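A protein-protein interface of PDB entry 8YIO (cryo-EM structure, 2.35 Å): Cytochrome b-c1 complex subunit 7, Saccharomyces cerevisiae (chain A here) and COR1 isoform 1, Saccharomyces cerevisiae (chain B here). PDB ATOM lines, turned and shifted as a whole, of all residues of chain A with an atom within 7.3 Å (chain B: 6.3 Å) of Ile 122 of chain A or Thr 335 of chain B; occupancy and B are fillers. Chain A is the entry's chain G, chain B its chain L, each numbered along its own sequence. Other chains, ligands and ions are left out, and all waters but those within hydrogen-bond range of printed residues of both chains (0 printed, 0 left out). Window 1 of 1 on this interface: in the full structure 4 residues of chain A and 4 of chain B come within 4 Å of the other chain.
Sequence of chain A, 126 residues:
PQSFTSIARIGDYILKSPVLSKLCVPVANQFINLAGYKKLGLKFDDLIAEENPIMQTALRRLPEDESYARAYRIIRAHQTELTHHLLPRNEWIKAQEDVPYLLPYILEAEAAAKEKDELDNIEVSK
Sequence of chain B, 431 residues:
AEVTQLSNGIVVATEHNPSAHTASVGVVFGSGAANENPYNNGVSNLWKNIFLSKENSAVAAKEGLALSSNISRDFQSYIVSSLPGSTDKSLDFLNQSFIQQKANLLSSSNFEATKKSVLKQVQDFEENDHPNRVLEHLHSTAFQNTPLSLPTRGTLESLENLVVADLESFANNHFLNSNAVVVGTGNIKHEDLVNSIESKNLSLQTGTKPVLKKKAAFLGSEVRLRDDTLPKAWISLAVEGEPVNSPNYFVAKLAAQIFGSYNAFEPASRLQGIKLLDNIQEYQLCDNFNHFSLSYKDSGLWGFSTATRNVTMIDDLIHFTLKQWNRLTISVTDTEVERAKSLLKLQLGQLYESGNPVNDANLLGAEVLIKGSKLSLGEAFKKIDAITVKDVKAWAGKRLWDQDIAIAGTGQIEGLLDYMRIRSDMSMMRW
The side-chain amino group (NZ) of Lys 275 of chain B lies within hydrogen-bond range of the backbone carbonyl oxygen (O) of Asp 120 of chain A (3.0 Å).
Among the printed residues, merely in contact across the chains: Val 124 of chain A with Asp 334 of chain B (3.4 Å), Ile 122 of chain A with Thr 335 of chain B (3.5 Å) and Val 124 of chain A with Thr 335 of chain B (3.8 Å).
Of the printed residues of chain B, Asp 120 of chain A touches Lys 275 (3.0 Å).
Of the printed residues of chain B, Ile 122 of chain A touches Thr 335.
Glu 123 of chain A touches none of the printed residues of chain B.
Printed residues of chain B within 4 Å of Val 124 of chain A: Asp 334 and Thr 335.
Of the printed residues of chain A, Lys 275 of chain B touches Asp 120.
Printed residues of chain A within 4 Å of Asp 334 of chain B: Val 124 (3.4 Å).
Thr 335 of chain B touches just these residues of chain A: Ile 122 (3.5 Å) and Val 124 (3.8 Å).
Glu 336 of chain B touches none of the printed residues of chain A.
The nearest residue of chain B that does not touch Ile 122 of chain A is Thr 333 of chain B (5.9 Å).
Hydrophobic or aromatic side chains of chain A that line the printed part of chain B: Ile 122 and Val 124.
Among the printed residues, 4 pairs touch across the chains.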
ATOM      1  N   ASP A 117      11.290 -13.895 -35.059  1.00  0.00           N
ATOM      2  CA  ASP A 117      11.566 -15.198 -34.464  1.00  0.00           C
ATOM      3  C   ASP A 117      13.061 -15.481 -34.381  1.00  0.00           C
ATOM      4  O   ASP A 117      13.506 -16.179 -33.465  1.00  0.00           O
ATOM      5  CB  ASP A 117      10.862 -16.288 -35.267  1.00  0.00           C
ATOM      6  CG  ASP A 117      10.892 -17.629 -34.575  1.00  0.00           C
ATOM      7  OD1 ASP A 117      10.106 -17.825 -33.628  1.00  0.00           O
ATOM      8  OD2 ASP A 117      11.703 -18.489 -34.979  1.00  0.00           O
ATOM      9  N   GLU A 118      13.850 -14.946 -35.312  1.00  0.00           N
ATOM     10  CA  GLU A 118      15.291 -15.149 -35.275  1.00  0.00           C
ATOM     11  C   GLU A 118      15.967 -14.291 -34.215  1.00  0.00           C
ATOM     12  O   GLU A 118      16.982 -14.705 -33.648  1.00  0.00           O
ATOM     13  CB  GLU A 118      15.897 -14.862 -36.648  1.00  0.00           C
ATOM     14  CG  GLU A 118      15.539 -15.894 -37.700  1.00  0.00           C
ATOM     15  CD  GLU A 118      16.046 -15.527 -39.079  1.00  0.00           C
ATOM     16  OE1 GLU A 118      16.000 -14.332 -39.437  1.00  0.00           O
ATOM     17  OE2 GLU A 118      16.488 -16.438 -39.809  1.00  0.00           O
ATOM     18  N   LEU A 119      15.430 -13.103 -33.937  1.00  0.00           N
ATOM     19  CA  LEU A 119      16.000 -12.240 -32.912  1.00  0.00           C
ATOM     20  C   LEU A 119      15.599 -12.655 -31.503  1.00  0.00           C
ATOM     21  O   LEU A 119      16.280 -12.277 -30.545  1.00  0.00           O
ATOM     22  CB  LEU A 119      15.589 -10.787 -33.157  1.00  0.00           C
ATOM     23  CG  LEU A 119      16.213 -10.065 -34.352  1.00  0.00           C
ATOM     24  CD1 LEU A 119      15.431  -8.813 -34.694  1.00  0.00           C
ATOM     25  CD2 LEU A 119      17.665  -9.724 -34.087  1.00  0.00           C
ATOM     26  N   ASP A 120      14.520 -13.420 -31.349  1.00  0.00           N
ATOM     27  CA  ASP A 120      14.064 -13.848 -30.034  1.00  0.00           C
ATOM     28  C   ASP A 120      14.749 -15.117 -29.540  1.00  0.00           C
ATOM     29  O   ASP A 120      14.755 -15.363 -28.330  1.00  0.00           O
ATOM     30  CB  ASP A 120      12.546 -14.063 -30.042  1.00  0.00           C
ATOM     31  CG  ASP A 120      11.768 -12.759 -30.004  1.00  0.00           C
ATOM     32  OD1 ASP A 120      12.386 -11.696 -29.796  1.00  0.00           O
ATOM     33  OD2 ASP A 120      10.534 -12.796 -30.183  1.00  0.00           O
ATOM     34  N   ASN A 121      15.324 -15.924 -30.433  1.00  0.00           N
ATOM     35  CA  ASN A 121      16.046 -17.148 -30.074  1.00  0.00           C
ATOM     36  C   ASN A 121      17.420 -17.050 -30.729  1.00  0.00           C
ATOM     37  O   ASN A 121      17.629 -17.593 -31.815  1.00  0.00           O
ATOM     38  CB  ASN A 121      15.299 -18.396 -30.534  1.00  0.00           C
ATOM     39  CG  ASN A 121      13.875 -18.454 -30.021  1.00  0.00           C
ATOM     40  OD1 ASN A 121      13.638 -18.669 -28.834  1.00  0.00           O
ATOM     41  ND2 ASN A 121      12.916 -18.279 -30.920  1.00  0.00           N
ATOM     42  N   ILE A 122      18.360 -16.383 -30.060  1.00  0.00           N
ATOM     43  CA  ILE A 122      19.574 -15.907 -30.712  1.00  0.00           C
ATOM     44  C   ILE A 122      20.773 -16.188 -29.811  1.00  0.00           C
ATOM     45  O   ILE A 122      20.651 -16.272 -28.586  1.00  0.00           O
ATOM     46  CB  ILE A 122      19.420 -14.401 -31.066  1.00  0.00           C
ATOM     47  CG1 ILE A 122      20.485 -13.916 -32.056  1.00  0.00           C
ATOM     48  CG2 ILE A 122      19.407 -13.532 -29.814  1.00  0.00           C
ATOM     49  CD1 ILE A 122      20.159 -12.578 -32.687  1.00  0.00           C
ATOM     50  N   GLU A 123      21.936 -16.373 -30.438  1.00  0.00           N
ATOM     51  CA  GLU A 123      23.209 -16.571 -29.758  1.00  0.00           C
ATOM     52  C   GLU A 123      24.037 -15.297 -29.857  1.00  0.00           C
ATOM     53  O   GLU A 123      23.755 -14.409 -30.666  1.00  0.00           O
ATOM     54  CB  GLU A 123      24.016 -17.719 -30.376  1.00  0.00           C
ATOM     55  CG  GLU A 123      23.423 -19.112 -30.257  1.00  0.00           C
ATOM     56  CD  GLU A 123      23.558 -19.696 -28.869  1.00  0.00           C
ATOM     57  OE1 GLU A 123      24.502 -19.313 -28.149  1.00  0.00           O
ATOM     58  OE2 GLU A 123      22.746 -20.568 -28.511  1.00  0.00           O
ATOM     59  N   VAL A 124      25.071 -15.220 -29.019  1.00  0.00           N
ATOM     60  CA  VAL A 124      26.082 -14.174 -29.081  1.00  0.00           C
ATOM     61  C   VAL A 124      27.455 -14.826 -28.963  1.00  0.00           C
ATOM     62  O   VAL A 124      27.586 -15.996 -28.597  1.00  0.00           O
ATOM     63  CB  VAL A 124      25.902 -13.092 -27.989  1.00  0.00           C
ATOM     64  CG1 VAL A 124      24.627 -12.277 -28.216  1.00  0.00           C
ATOM     65  CG2 VAL A 124      25.890 -13.729 -26.610  1.00  0.00           C
ATOM     66  N   LYS B 275      11.319 -10.412 -22.876  1.00  0.00           N
ATOM     67  CA  LYS B 275      10.376 -11.490 -23.165  1.00  0.00           C
ATOM     68  C   LYS B 275       9.047 -11.327 -22.439  1.00  0.00           C
ATOM     69  O   LYS B 275       8.076 -11.995 -22.806  1.00  0.00           O
ATOM     70  CB  LYS B 275      10.990 -12.843 -22.807  1.00  0.00           C
ATOM     71  CG  LYS B 275      12.198 -13.227 -23.638  1.00  0.00           C
ATOM     72  CD  LYS B 275      12.561 -14.686 -23.435  1.00  0.00           C
ATOM     73  CE  LYS B 275      13.936 -15.004 -23.997  1.00  0.00           C
ATOM     74  NZ  LYS B 275      14.019 -14.740 -25.457  1.00  0.00           N
ATOM     75  N   THR B 333      19.122 -16.844 -20.061  1.00  0.00           N
ATOM     76  CA  THR B 333      20.026 -17.117 -21.167  1.00  0.00           C
ATOM     77  C   THR B 333      21.196 -16.135 -21.185  1.00  0.00           C
ATOM     78  O   THR B 333      21.203 -15.116 -20.495  1.00  0.00           O
ATOM     79  CB  THR B 333      19.280 -17.079 -22.501  1.00  0.00           C
ATOM     80  OG1 THR B 333      19.090 -15.718 -22.905  1.00  0.00           O
ATOM     81  CG2 THR B 333      17.926 -17.755 -22.378  1.00  0.00           C
ATOM     82  N   ASP B 334      22.192 -16.456 -22.011  1.00  0.00           N
ATOM     83  CA  ASP B 334      23.418 -15.670 -22.069  1.00  0.00           C
ATOM     84  C   ASP B 334      23.237 -14.385 -22.867  1.00  0.00           C
ATOM     85  O   ASP B 334      23.916 -13.393 -22.590  1.00  0.00           O
ATOM     86  CB  ASP B 334      24.547 -16.523 -22.649  1.00  0.00           C
ATOM     87  CG  ASP B 334      25.898 -15.846 -22.594  1.00  0.00           C
ATOM     88  OD1 ASP B 334      26.591 -15.969 -21.561  1.00  0.00           O
ATOM     89  OD2 ASP B 334      26.281 -15.189 -23.585  1.00  0.00           O
ATOM     90  N   THR B 335      22.331 -14.370 -23.847  1.00  0.00           N
ATOM     91  CA  THR B 335      22.088 -13.158 -24.619  1.00  0.00           C
ATOM     92  C   THR B 335      21.270 -12.119 -23.853  1.00  0.00           C
ATOM     93  O   THR B 335      21.363 -10.929 -24.165  1.00  0.00           O
ATOM     94  CB  THR B 335      21.406 -13.501 -25.955  1.00  0.00           C
ATOM     95  OG1 THR B 335      21.148 -12.301 -26.691  1.00  0.00           O
ATOM     96  CG2 THR B 335      20.099 -14.248 -25.744  1.00  0.00           C
ATOM     97  N   GLU B 336      20.483 -12.535 -22.856  1.00  0.00           N
ATOM     98  CA  GLU B 336      19.800 -11.565 -22.004  1.00  0.00           C
ATOM     99  C   GLU B 336      20.770 -10.874 -21.056  1.00  0.00           C
ATOM    100  O   GLU B 336      20.581  -9.699 -20.730  1.00  0.00           O
ATOM    101  CB  GLU B 336      18.685 -12.245 -21.210  1.00  0.00           C
ATOM    102  CG  GLU B 336      17.578 -12.813 -22.069  1.00  0.00           C
ATOM    103  CD  GLU B 336      16.512 -13.525 -21.264  1.00  0.00           C
ATOM    104  OE1 GLU B 336      15.595 -12.849 -20.762  1.00  0.00           O
ATOM    105  OE2 GLU B 336      16.585 -14.764 -21.138  1.00  0.00           O
ATOM    106  N   VAL B 337      21.813 -11.582 -20.618  1.00  0.00           N
ATOM    107  CA  VAL B 337      22.783 -11.018 -19.686  1.00  0.00           C
ATOM    108  C   VAL B 337      23.686 -10.009 -20.392  1.00  0.00           C
ATOM    109  O   VAL B 337      24.043  -8.972 -19.820  1.00  0.00           O
ATOM    110  CB  VAL B 337      23.579 -12.161 -19.020  1.00  0.00           C
ATOM    111  CG1 VAL B 337      24.669 -11.642 -18.099  1.00  0.00           C
ATOM    112  CG2 VAL B 337      22.643 -13.066 -18.244  1.00  0.00           C
ATOM    113  N   GLU B 338      24.042 -10.274 -21.653  1.00  0.00           N
ATOM    114  CA  GLU B 338      24.893  -9.347 -22.399  1.00  0.00           C
ATOM    115  C   GLU B 338      24.152  -8.065 -22.757  1.00  0.00           C
ATOM    116  O   GLU B 338      24.762  -6.993 -22.817  1.00  0.00           O
ATOM    117  CB  GLU B 338      25.428 -10.010 -23.671  1.00  0.00           C
ATOM    118  CG  GLU B 338      26.275 -11.244 -23.446  1.00  0.00           C
ATOM    119  CD  GLU B 338      27.440 -11.003 -22.507  1.00  0.00           C
ATOM    120  OE1 GLU B 338      28.181 -10.020 -22.708  1.00  0.00           O
ATOM    121  OE2 GLU B 338      27.616 -11.803 -21.565  1.00  0.00           O
ATOM    122  N   ARG B 339      22.845  -8.160 -23.018  1.00  0.00           N
ATOM    123  CA  ARG B 339      22.045  -6.967 -23.284  1.00  0.00           C
ATOM    124  C   ARG B 339      21.922  -6.096 -22.038  1.00  0.00           C
ATOM    125  O   ARG B 339      22.017  -4.867 -22.123  1.00  0.00           O
ATOM    126  CB  ARG B 339      20.662  -7.368 -23.801  1.00  0.00           C
ATOM    127  CG  ARG B 339      19.705  -6.205 -24.034  1.00  0.00           C
ATOM    128  CD  ARG B 339      18.265  -6.677 -24.150  1.00  0.00           C
ATOM    129  NE  ARG B 339      17.312  -5.571 -24.153  1.00  0.00           N
ATOM    130  CZ  ARG B 339      16.716  -5.081 -23.069  1.00  0.00           C
ATOM    131  NH1 ARG B 339      15.864  -4.072 -23.179  1.00  0.00           N
ATOM    132  NH2 ARG B 339      16.972  -5.590 -21.875  1.00  0.00           N
ATOM    133  N   ALA B 340      21.740  -6.718 -20.872  1.00  0.00           N
ATOM    134  CA  ALA B 340      21.623  -5.972 -19.626  1.00  0.00           C
ATOM    135  C   ALA B 340      22.939  -5.340 -19.195  1.00  0.00           C
ATOM    136  O   ALA B 340      22.918  -4.361 -18.447  1.00  0.00           O
ATOM    137  CB  ALA B 340      21.092  -6.879 -18.518  1.00  0.00           C
